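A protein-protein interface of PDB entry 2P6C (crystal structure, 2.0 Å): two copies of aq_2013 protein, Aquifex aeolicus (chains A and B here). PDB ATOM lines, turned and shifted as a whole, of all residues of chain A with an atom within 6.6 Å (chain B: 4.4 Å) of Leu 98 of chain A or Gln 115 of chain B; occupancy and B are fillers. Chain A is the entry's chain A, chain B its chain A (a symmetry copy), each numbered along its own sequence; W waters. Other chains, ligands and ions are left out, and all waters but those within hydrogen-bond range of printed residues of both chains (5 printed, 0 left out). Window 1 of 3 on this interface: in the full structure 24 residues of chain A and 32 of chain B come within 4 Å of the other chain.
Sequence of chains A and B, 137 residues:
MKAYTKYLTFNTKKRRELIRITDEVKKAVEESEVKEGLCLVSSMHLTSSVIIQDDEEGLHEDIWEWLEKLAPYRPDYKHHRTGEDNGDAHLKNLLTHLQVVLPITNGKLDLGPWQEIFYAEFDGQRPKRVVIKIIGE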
ATOM      1  N   VAL A  41      26.178  29.550   5.070  1.00  0.00           N
ATOM      2  CA  VAL A  41      26.622  28.252   5.574  1.00  0.00           C
ATOM      3  C   VAL A  41      26.782  28.473   7.063  1.00  0.00           C
ATOM      4  O   VAL A  41      27.677  29.187   7.512  1.00  0.00           O
ATOM      5  CB  VAL A  41      27.949  27.844   4.946  1.00  0.00           C
ATOM      6  CG1 VAL A  41      28.273  26.409   5.312  1.00  0.00           C
ATOM      7  CG2 VAL A  41      27.878  28.023   3.434  1.00  0.00           C
ATOM      8  N   SER A  42      25.903  27.849   7.830  1.00  0.00           N
ATOM      9  CA  SER A  42      25.878  28.070   9.259  1.00  0.00           C
ATOM     10  C   SER A  42      25.690  26.818  10.100  1.00  0.00           C
ATOM     11  O   SER A  42      24.931  25.914   9.737  1.00  0.00           O
ATOM     12  CB  SER A  42      24.731  29.046   9.551  1.00  0.00           C
ATOM     13  OG  SER A  42      24.705  29.444  10.903  1.00  0.00           O
ATOM     14  N   SER A  43      26.383  26.767  11.232  1.00  0.00           N
ATOM     15  CA  SER A  43      26.184  25.678  12.165  1.00  0.00           C
ATOM     16  C   SER A  43      24.871  25.856  12.876  1.00  0.00           C
ATOM     17  O   SER A  43      24.505  26.946  13.274  1.00  0.00           O
ATOM     18  CB  SER A  43      27.301  25.704  13.206  1.00  0.00           C
ATOM     19  OG  SER A  43      26.978  24.758  14.233  1.00  0.00           O
ATOM     20  N   MET A  44      24.154  24.735  13.018  1.00  0.00           N
ATOM     21  CA  MET A  44      22.874  24.798  13.728  1.00  0.00           C
ATOM     22  C   MET A  44      23.044  24.544  15.229  1.00  0.00           C
ATOM     23  O   MET A  44      22.072  24.452  15.965  1.00  0.00           O
ATOM     24  CB  MET A  44      21.927  23.777  13.107  1.00  0.00           C
ATOM     25  CG  MET A  44      21.746  24.007  11.599  1.00  0.00           C
ATOM     26  SD  MET A  44      20.261  23.218  10.923  1.00  0.00           S
ATOM     27  CE  MET A  44      19.011  24.362  11.533  1.00  0.00           C
ATOM     28  N   HIS A  45      24.294  24.466  15.673  1.00  0.00           N
ATOM     29  CA  HIS A  45      24.582  24.211  17.073  1.00  0.00           C
ATOM     30  C   HIS A  45      25.453  25.306  17.684  1.00  0.00           C
ATOM     31  O   HIS A  45      26.149  26.040  16.983  1.00  0.00           O
ATOM     32  CB  HIS A  45      25.259  22.834  17.207  1.00  0.00           C
ATOM     33  CG  HIS A  45      24.461  21.724  16.599  1.00  0.00           C
ATOM     34  ND1 HIS A  45      23.640  20.909  17.347  1.00  0.00           N
ATOM     35  CD2 HIS A  45      24.252  21.382  15.304  1.00  0.00           C
ATOM     36  CE1 HIS A  45      22.953  20.119  16.542  1.00  0.00           C
ATOM     37  NE2 HIS A  45      23.305  20.386  15.297  1.00  0.00           N
ATOM     38  N   LEU A  46      25.433  25.390  19.007  1.00  0.00           N
ATOM     39  CA  LEU A  46      26.153  26.406  19.815  1.00  0.00           C
ATOM     40  C   LEU A  46      27.584  25.916  20.144  1.00  0.00           C
ATOM     41  O   LEU A  46      28.390  26.583  20.781  1.00  0.00           O
ATOM     42  CB  LEU A  46      25.449  26.636  21.196  1.00  0.00           C
ATOM     43  CG  LEU A  46      24.112  27.467  21.155  1.00  0.00           C
ATOM     44  CD1 LEU A  46      24.152  28.795  20.398  1.00  0.00           C
ATOM     45  CD2 LEU A  46      22.937  26.685  20.591  1.00  0.00           C
ATOM     46  N   SER A  48      29.743  24.342  17.835  1.00  0.00           N
ATOM     47  CA  SER A  48      30.432  24.144  16.577  1.00  0.00           C
ATOM     48  C   SER A  48      30.166  25.367  15.706  1.00  0.00           C
ATOM     49  O   SER A  48      29.158  26.061  15.881  1.00  0.00           O
ATOM     50  CB  SER A  48      29.922  22.875  15.884  1.00  0.00           C
ATOM     51  OG  SER A  48      28.551  22.969  15.532  1.00  0.00           O
ATOM     52  N   SER A  49      31.071  25.624  14.766  1.00  0.00           N
ATOM     53  CA  SER A  49      30.933  26.765  13.838  1.00  0.00           C
ATOM     54  C   SER A  49      31.406  26.411  12.414  1.00  0.00           C
ATOM     55  O   SER A  49      32.222  25.511  12.217  1.00  0.00           O
ATOM     56  CB  SER A  49      31.785  27.945  14.368  1.00  0.00           C
ATOM     57  OG  SER A  49      31.293  28.410  15.634  1.00  0.00           O
ATOM     58  N   VAL A  50      30.770  27.096  11.393  1.00  0.00           N
ATOM     59  CA  VAL A  50      31.344  27.222  10.042  1.00  0.00           C
ATOM     60  C   VAL A  50      32.168  28.478   9.989  1.00  0.00           C
ATOM     61  O   VAL A  50      31.737  29.583  10.305  1.00  0.00           O
ATOM     62  CB  VAL A  50      30.251  27.299   8.965  1.00  0.00           C
ATOM     63  CG1 VAL A  50      30.898  27.452   7.568  1.00  0.00           C
ATOM     64  CG2 VAL A  50      29.407  26.042   8.966  1.00  0.00           C
ATOM     65  N   ILE A  51      33.449  28.219   9.644  1.00  0.00           N
ATOM     66  CA  ILE A  51      34.524  29.246   9.578  1.00  0.00           C
ATOM     67  C   ILE A  51      35.175  29.124   8.201  1.00  0.00           C
ATOM     68  O   ILE A  51      35.133  28.084   7.556  1.00  0.00           O
ATOM     69  CB  ILE A  51      35.595  29.200  10.778  1.00  0.00           C
ATOM     70  CG1 ILE A  51      36.385  27.891  10.711  1.00  0.00           C
ATOM     71  CG2 ILE A  51      34.863  29.230  12.132  1.00  0.00           C
ATOM     72  CD1 ILE A  51      37.618  27.900  11.617  1.00  0.00           C
ATOM     73  N   ASN A  93      32.473  28.952  19.994  1.00  0.00           N
ATOM     74  CA  ASN A  93      31.450  29.229  18.978  1.00  0.00           C
ATOM     75  C   ASN A  93      31.213  30.742  18.889  1.00  0.00           C
ATOM     76  O   ASN A  93      31.068  31.338  17.833  1.00  0.00           O
ATOM     77  CB  ASN A  93      30.161  28.493  19.381  1.00  0.00           C
ATOM     78  CG  ASN A  93      28.959  29.023  18.638  1.00  0.00           C
ATOM     79  OD1 ASN A  93      28.223  29.880  19.121  1.00  0.00           O
ATOM     80  ND2 ASN A  93      28.765  28.495  17.417  1.00  0.00           N
ATOM     81  N   LEU A  94      31.204  31.341  20.079  1.00  0.00           N
ATOM     82  CA  LEU A  94      31.057  32.790  20.126  1.00  0.00           C
ATOM     83  C   LEU A  94      32.230  33.465  19.415  1.00  0.00           C
ATOM     84  O   LEU A  94      32.063  34.349  18.585  1.00  0.00           O
ATOM     85  CB  LEU A  94      31.004  33.231  21.599  1.00  0.00           C
ATOM     86  CG  LEU A  94      29.695  33.946  21.982  1.00  0.00           C
ATOM     87  CD1 LEU A  94      29.847  34.817  23.230  1.00  0.00           C
ATOM     88  CD2 LEU A  94      29.174  34.864  20.877  1.00  0.00           C
ATOM     89  N   THR A  96      34.639  32.325  17.225  1.00  0.00           N
ATOM     90  CA  THR A  96      34.806  32.075  15.797  1.00  0.00           C
ATOM     91  C   THR A  96      33.607  32.475  14.956  1.00  0.00           C
ATOM     92  O   THR A  96      33.719  32.599  13.742  1.00  0.00           O
ATOM     93  CB  THR A  96      35.067  30.571  15.504  1.00  0.00           C
ATOM     94  OG1 THR A  96      34.018  29.779  16.077  1.00  0.00           O
ATOM     95  CG2 THR A  96      36.397  30.129  16.069  1.00  0.00           C
ATOM     96  N   HIS A  97      32.467  32.672  15.603  1.00  0.00           N
ATOM     97  CA  HIS A  97      31.211  33.002  14.925  1.00  0.00           C
ATOM     98  C   HIS A  97      30.663  31.761  14.227  1.00  0.00           C
ATOM     99  O   HIS A  97      31.367  31.095  13.468  1.00  0.00           O
ATOM    100  CB  HIS A  97      31.376  34.112  13.892  1.00  0.00           C
ATOM    101  CG  HIS A  97      30.084  34.797  13.557  1.00  0.00           C
ATOM    102  ND1 HIS A  97      29.229  35.269  14.529  1.00  0.00           N
ATOM    103  CD2 HIS A  97      29.503  35.091  12.368  1.00  0.00           C
ATOM    104  CE1 HIS A  97      28.177  35.825  13.956  1.00  0.00           C
ATOM    105  NE2 HIS A  97      28.318  35.731  12.645  1.00  0.00           N
ATOM    106  N   LEU A  98      29.388  31.477  14.458  1.00  0.00           N
ATOM    107  CA  LEU A  98      28.718  30.251  13.949  1.00  0.00           C
ATOM    108  C   LEU A  98      28.616  30.135  12.400  1.00  0.00           C
ATOM    109  O   LEU A  98      28.436  29.061  11.841  1.00  0.00           O
ATOM    110  CB  LEU A  98      27.321  30.167  14.569  1.00  0.00           C
ATOM    111  CG  LEU A  98      26.256  30.910  13.752  1.00  0.00           C
ATOM    112  CD1 LEU A  98      24.837  30.476  14.122  1.00  0.00           C
ATOM    113  CD2 LEU A  98      26.307  32.424  13.956  1.00  0.00           C
ATOM    114  N   GLN A  99      28.738  31.229  11.651  1.00  0.00           N
ATOM    115  CA  GLN A  99      28.489  31.164  10.215  1.00  0.00           C
ATOM    116  C   GLN A  99      29.324  32.064   9.296  1.00  0.00           C
ATOM    117  O   GLN A  99      30.129  32.883   9.735  1.00  0.00           O
ATOM    118  CB  GLN A  99      27.019  31.532   9.993  1.00  0.00           C
ATOM    119  CG  GLN A  99      26.784  33.045  10.212  1.00  0.00           C
ATOM    120  CD  GLN A  99      25.325  33.466  10.370  1.00  0.00           C
ATOM    121  OE1 GLN A  99      24.998  34.649  10.225  1.00  0.00           O
ATOM    122  NE2 GLN A  99      24.449  32.514  10.688  1.00  0.00           N
ATOM    123  N   VAL A 100      29.072  31.902   7.999  1.00  0.00           N
ATOM    124  CA  VAL A 100      29.723  32.699   6.887  1.00  0.00           C
ATOM    125  C   VAL A 100      28.696  32.819   5.805  1.00  0.00           C
ATOM    126  O   VAL A 100      27.829  31.971   5.638  1.00  0.00           O
ATOM    127  CB  VAL A 100      31.115  32.172   6.250  1.00  0.00           C
ATOM    128  CG1 VAL A 100      32.205  32.158   7.319  1.00  0.00           C
ATOM    129  CG2 VAL A 100      30.934  30.767   5.706  1.00  0.00           C
ATOM    130  N   ILE B  52      23.631  34.655  18.724  1.00  0.00           N
ATOM    131  CA  ILE B  52      22.896  33.423  18.928  1.00  0.00           C
ATOM    132  C   ILE B  52      23.617  32.614  19.963  1.00  0.00           C
ATOM    133  O   ILE B  52      24.787  32.278  19.824  1.00  0.00           O
ATOM    134  CB  ILE B  52      22.832  32.616  17.620  1.00  0.00           C
ATOM    135  CG1 ILE B  52      21.809  33.249  16.672  1.00  0.00           C
ATOM    136  CG2 ILE B  52      22.366  31.179  17.915  1.00  0.00           C
ATOM    137  CD1 ILE B  52      21.839  32.626  15.274  1.00  0.00           C
ATOM    138  N   GLN B  53      22.930  32.411  21.087  1.00  0.00           N
ATOM    139  CA  GLN B  53      23.375  31.603  22.204  1.00  0.00           C
ATOM    140  C   GLN B  53      22.297  30.599  22.516  1.00  0.00           C
ATOM    141  O   GLN B  53      21.342  30.474  21.799  1.00  0.00           O
ATOM    142  CB  GLN B  53      23.499  32.483  23.415  1.00  0.00           C
ATOM    143  CG  GLN B  53      24.647  33.441  23.242  1.00  0.00           C
ATOM    144  CD  GLN B  53      25.950  32.683  23.305  1.00  0.00           C
ATOM    145  OE1 GLN B  53      26.563  32.510  24.346  1.00  0.00           O
ATOM    146  NE2 GLN B  53      26.425  32.314  22.099  1.00  0.00           N
ATOM    147  N   VAL B 100      23.770  38.407  12.827  1.00  0.00           N
ATOM    148  CA  VAL B 100      23.534  36.959  12.452  1.00  0.00           C
ATOM    149  C   VAL B 100      22.627  36.981  11.261  1.00  0.00           C
ATOM    150  O   VAL B 100      21.827  37.888  11.073  1.00  0.00           O
ATOM    151  CB  VAL B 100      22.938  35.944  13.562  1.00  0.00           C
ATOM    152  CG1 VAL B 100      23.912  35.820  14.732  1.00  0.00           C
ATOM    153  CG2 VAL B 100      21.608  36.464  14.077  1.00  0.00           C
ATOM    154  N   LEU B 111      15.916  27.294  12.750  1.00  0.00           N
ATOM    155  CA  LEU B 111      16.824  27.271  13.893  1.00  0.00           C
ATOM    156  C   LEU B 111      17.154  25.872  14.404  1.00  0.00           C
ATOM    157  O   LEU B 111      16.376  24.933  14.346  1.00  0.00           O
ATOM    158  CB  LEU B 111      16.159  27.997  15.054  1.00  0.00           C
ATOM    159  CG  LEU B 111      16.118  29.501  14.845  1.00  0.00           C
ATOM    160  CD1 LEU B 111      15.607  30.226  16.087  1.00  0.00           C
ATOM    161  CD2 LEU B 111      17.482  30.104  14.516  1.00  0.00           C
ATOM    162  N   GLY B 112      18.370  25.764  14.985  1.00  0.00           N
ATOM    163  CA  GLY B 112      18.830  24.512  15.595  1.00  0.00           C
ATOM    164  C   GLY B 112      18.020  24.158  16.866  1.00  0.00           C
ATOM    165  O   GLY B 112      17.214  24.937  17.351  1.00  0.00           O
ATOM    166  N   PRO B 113      18.190  22.963  17.460  1.00  0.00           N
ATOM    167  CA  PRO B 113      17.394  22.596  18.638  1.00  0.00           C
ATOM    168  C   PRO B 113      17.544  23.478  19.869  1.00  0.00           C
ATOM    169  O   PRO B 113      16.636  23.554  20.692  1.00  0.00           O
ATOM    170  CB  PRO B 113      17.819  21.152  18.912  1.00  0.00           C
ATOM    171  CG  PRO B 113      19.169  20.931  18.302  1.00  0.00           C
ATOM    172  CD  PRO B 113      19.173  21.909  17.140  1.00  0.00           C
ATOM    173  N   TRP B 114      18.682  24.149  20.004  1.00  0.00           N
ATOM    174  CA  TRP B 114      18.888  24.983  21.176  1.00  0.00           C
ATOM    175  C   TRP B 114      19.161  26.459  20.879  1.00  0.00           C
ATOM    176  O   TRP B 114      19.226  27.268  21.803  1.00  0.00           O
ATOM    177  CB  TRP B 114      20.025  24.396  22.025  1.00  0.00           C
ATOM    178  CG  TRP B 114      19.731  23.005  22.548  1.00  0.00           C
ATOM    179  CD1 TRP B 114      20.469  21.866  22.327  1.00  0.00           C
ATOM    180  CD2 TRP B 114      18.645  22.616  23.397  1.00  0.00           C
ATOM    181  NE1 TRP B 114      19.907  20.798  22.988  1.00  0.00           N
ATOM    182  CE2 TRP B 114      18.787  21.231  23.655  1.00  0.00           C
ATOM    183  CE3 TRP B 114      17.565  23.303  23.972  1.00  0.00           C
ATOM    184  CZ2 TRP B 114      17.884  20.522  24.462  1.00  0.00           C
ATOM    185  CZ3 TRP B 114      16.670  22.599  24.772  1.00  0.00           C
ATOM    186  CH2 TRP B 114      16.835  21.223  25.012  1.00  0.00           C
ATOM    187  N   GLN B 115      19.303  26.817  19.605  1.00  0.00           N
ATOM    188  CA  GLN B 115      19.581  28.200  19.192  1.00  0.00           C
ATOM    189  C   GLN B 115      18.489  29.192  19.646  1.00  0.00           C
ATOM    190  O   GLN B 115      17.298  28.957  19.494  1.00  0.00           O
ATOM    191  CB  GLN B 115      19.723  28.230  17.664  1.00  0.00           C
ATOM    192  CG  GLN B 115      21.099  27.753  17.187  1.00  0.00           C
ATOM    193  CD  GLN B 115      21.205  27.902  15.682  1.00  0.00           C
ATOM    194  OE1 GLN B 115      20.261  27.731  14.930  1.00  0.00           O
ATOM    195  NE2 GLN B 115      22.439  28.239  15.256  1.00  0.00           N
ATOM    196  N   GLU B 116      18.917  30.328  20.177  1.00  0.00           N
ATOM    197  CA  GLU B 116      18.019  31.399  20.588  1.00  0.00           C
ATOM    198  C   GLU B 116      18.722  32.693  20.188  1.00  0.00           C
ATOM    199  O   GLU B 116      19.930  32.821  20.360  1.00  0.00           O
ATOM    200  CB  GLU B 116      17.801  31.367  22.103  1.00  0.00           C
ATOM    201  CG  GLU B 116      17.070  32.592  22.671  1.00  0.00           C
ATOM    202  CD  GLU B 116      15.568  32.553  22.446  1.00  0.00           C
ATOM    203  OE1 GLU B 116      15.055  31.523  21.955  1.00  0.00           O
ATOM    204  OE2 GLU B 116      14.894  33.557  22.771  1.00  0.00           O
HETATM  205  O   HOH W   1      26.308  31.177  17.932  1.00  0.00           O
HETATM  206  O   HOH W   2      28.013  30.135  21.785  1.00  0.00           O
HETATM  207  O   HOH W   3      24.414  28.892  17.039  1.00  0.00           O
HETATM  208  O   HOH W   4      21.329  24.100  18.657  1.00  0.00           O
HETATM  209  O   HOH W   5      22.410  28.352  12.011  1.00  0.00           O
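The backbone carbonyl oxygen of Ser 43 of chain A is in hydrogen-bond range of the side-chain amide nitrogen of Gln 115 of chain B (3.1 Å).
The side-chain amide nitrogen (NE2) of Gln 99 of chain A lies within hydrogen-bond range of the side-chain hydroxyl (OG) of Ser 42 of chain A, 3.1 Å away.
The side-chain hydroxyl (OG) of Ser 43 of chain A is in hydrogen-bond range of the side-chain hydroxyl (OG) of Ser 48 of chain A (2.7 Å).
The backbone NH (N) of Ser 43 of chain A is in hydrogen-bond range of the backbone carbonyl oxygen (O) of Leu 98 of chain A, at 3.1 Å.
N of Val 50 of chain A is in hydrogen-bond range of O of Leu 98 of chain A.
The backbone carbonyl oxygen (O) of Gln 53 of chain B lies within hydrogen-bond range of the backbone NH (N) of Glu 116 of chain B, 2.9 Å away.
N of Gly 112 of chain B is in hydrogen-bond range of OE1 of Gln 115 of chain B (2.7 Å).
Met 44 of chain A touches Leu 111 of chain B.
CA of Gly 112 of chain B touches O of Met 44 of chain A, 3.3 Å away.
Met 44 of chain A touches Gln 115 of chain B.
CD1 of Leu 46 of chain A touches O of Ile 52 of chain B, at 3.6 Å.
Gln 53 of chain B touches Leu 46 of chain A (C to CD1, 3.3 Å).
Leu 46 of chain A touches Trp 114 of chain B.
Gln 115 of chain B touches Leu 46 of chain A.
CG of Leu 94 of chain A touches NE2 of Gln 53 of chain B, at 3.7 Å.
Leu 98 of chain A touches Ile 52 of chain B.
OE1 of Gln 99 of chain A touches C of Val 100 of chain B (3.5 Å).
Leu 98 of chain A touches just these residues of chain B: Ile 52 and Gln 115.
Printed residues of chain A within 4 Å of Gln 115 of chain B: Ser 43 (3.1 Å), Met 44 (3.6 Å), Leu 46 (3.8 Å) and Leu 98 (3.5 Å).
Of the printed residues of chain B, Met 44 of chain A touches Leu 111, Gly 112 and Gln 115.
Of the printed residues of chain B, Leu 94 of chain A touches Gln 53 (3.7 Å).
Printed residues of chain A within 4 Å of Gln 53 of chain B: Leu 46 and Leu 94.
Printed residues of chain A within 4 Å of Leu 111 of chain B: Met 44.
Ser 48 of chain A touches none of the printed residues of chain B.
The nearest residue of chain B that does not touch Leu 98 of chain A is Val 100 of chain B (4.2 Å).
Hydrophobic or aromatic side chains of chain A within 4 Å of the printed part of chain B: Met 44, Leu 46, Leu 94 and Leu 98.
Of the 9 printed residues of chain B, 7 touch a printed residue of chain A.
Printed residues of chain B that touch a printed residue of chain A: Ile 52, Gln 53, Val 100, Leu 111, Gly 112, Trp 114 and Gln 115.
Hydrophobic or aromatic side chains of chain B that line the printed part of chain A: Ile 52 and Trp 114.
Along chain B the printed residues that touch a printed residue of chain A span positions 52 to 115.
Among the printed residues, 12 pairs touch across the chains.
Among the printed residues, no Asp or Glu carboxylate lies within 4 Å of a Lys or Arg side-chain nitrogen of the other chain.
Position printed for both chains: 100.
Of the 12 pairs that touch across the chains among the printed residues, none has its exchanged pair printed and touching as well.
Water W1 bridges OD1 of Asn 93 of chain A and O of Ile 52 of chain B.
Water W2 bridges OD1 of Asn 93 of chain A (2.7 Å) and NE2 of Gln 53 of chain B (2.7 Å).
Water W3 bridges the side-chain amide nitrogen of Gln 115 of chain B and the backbone carbonyl oxygen of His 45 of chain A.
Water W5 lies within hydrogen-bond range of the side-chain hydroxyl (OG) of Ser 42 of chain A (2.8 Å), the backbone carbonyl oxygen (O) of Ser 43 of chain A (2.8 Å) and the side-chain amide nitrogen (NE2) of Gln 115 of chain B (3.2 Å).
Water W4 lies within hydrogen-bond range of O of Met 44 of chain A and N of Trp 114 of chain B.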
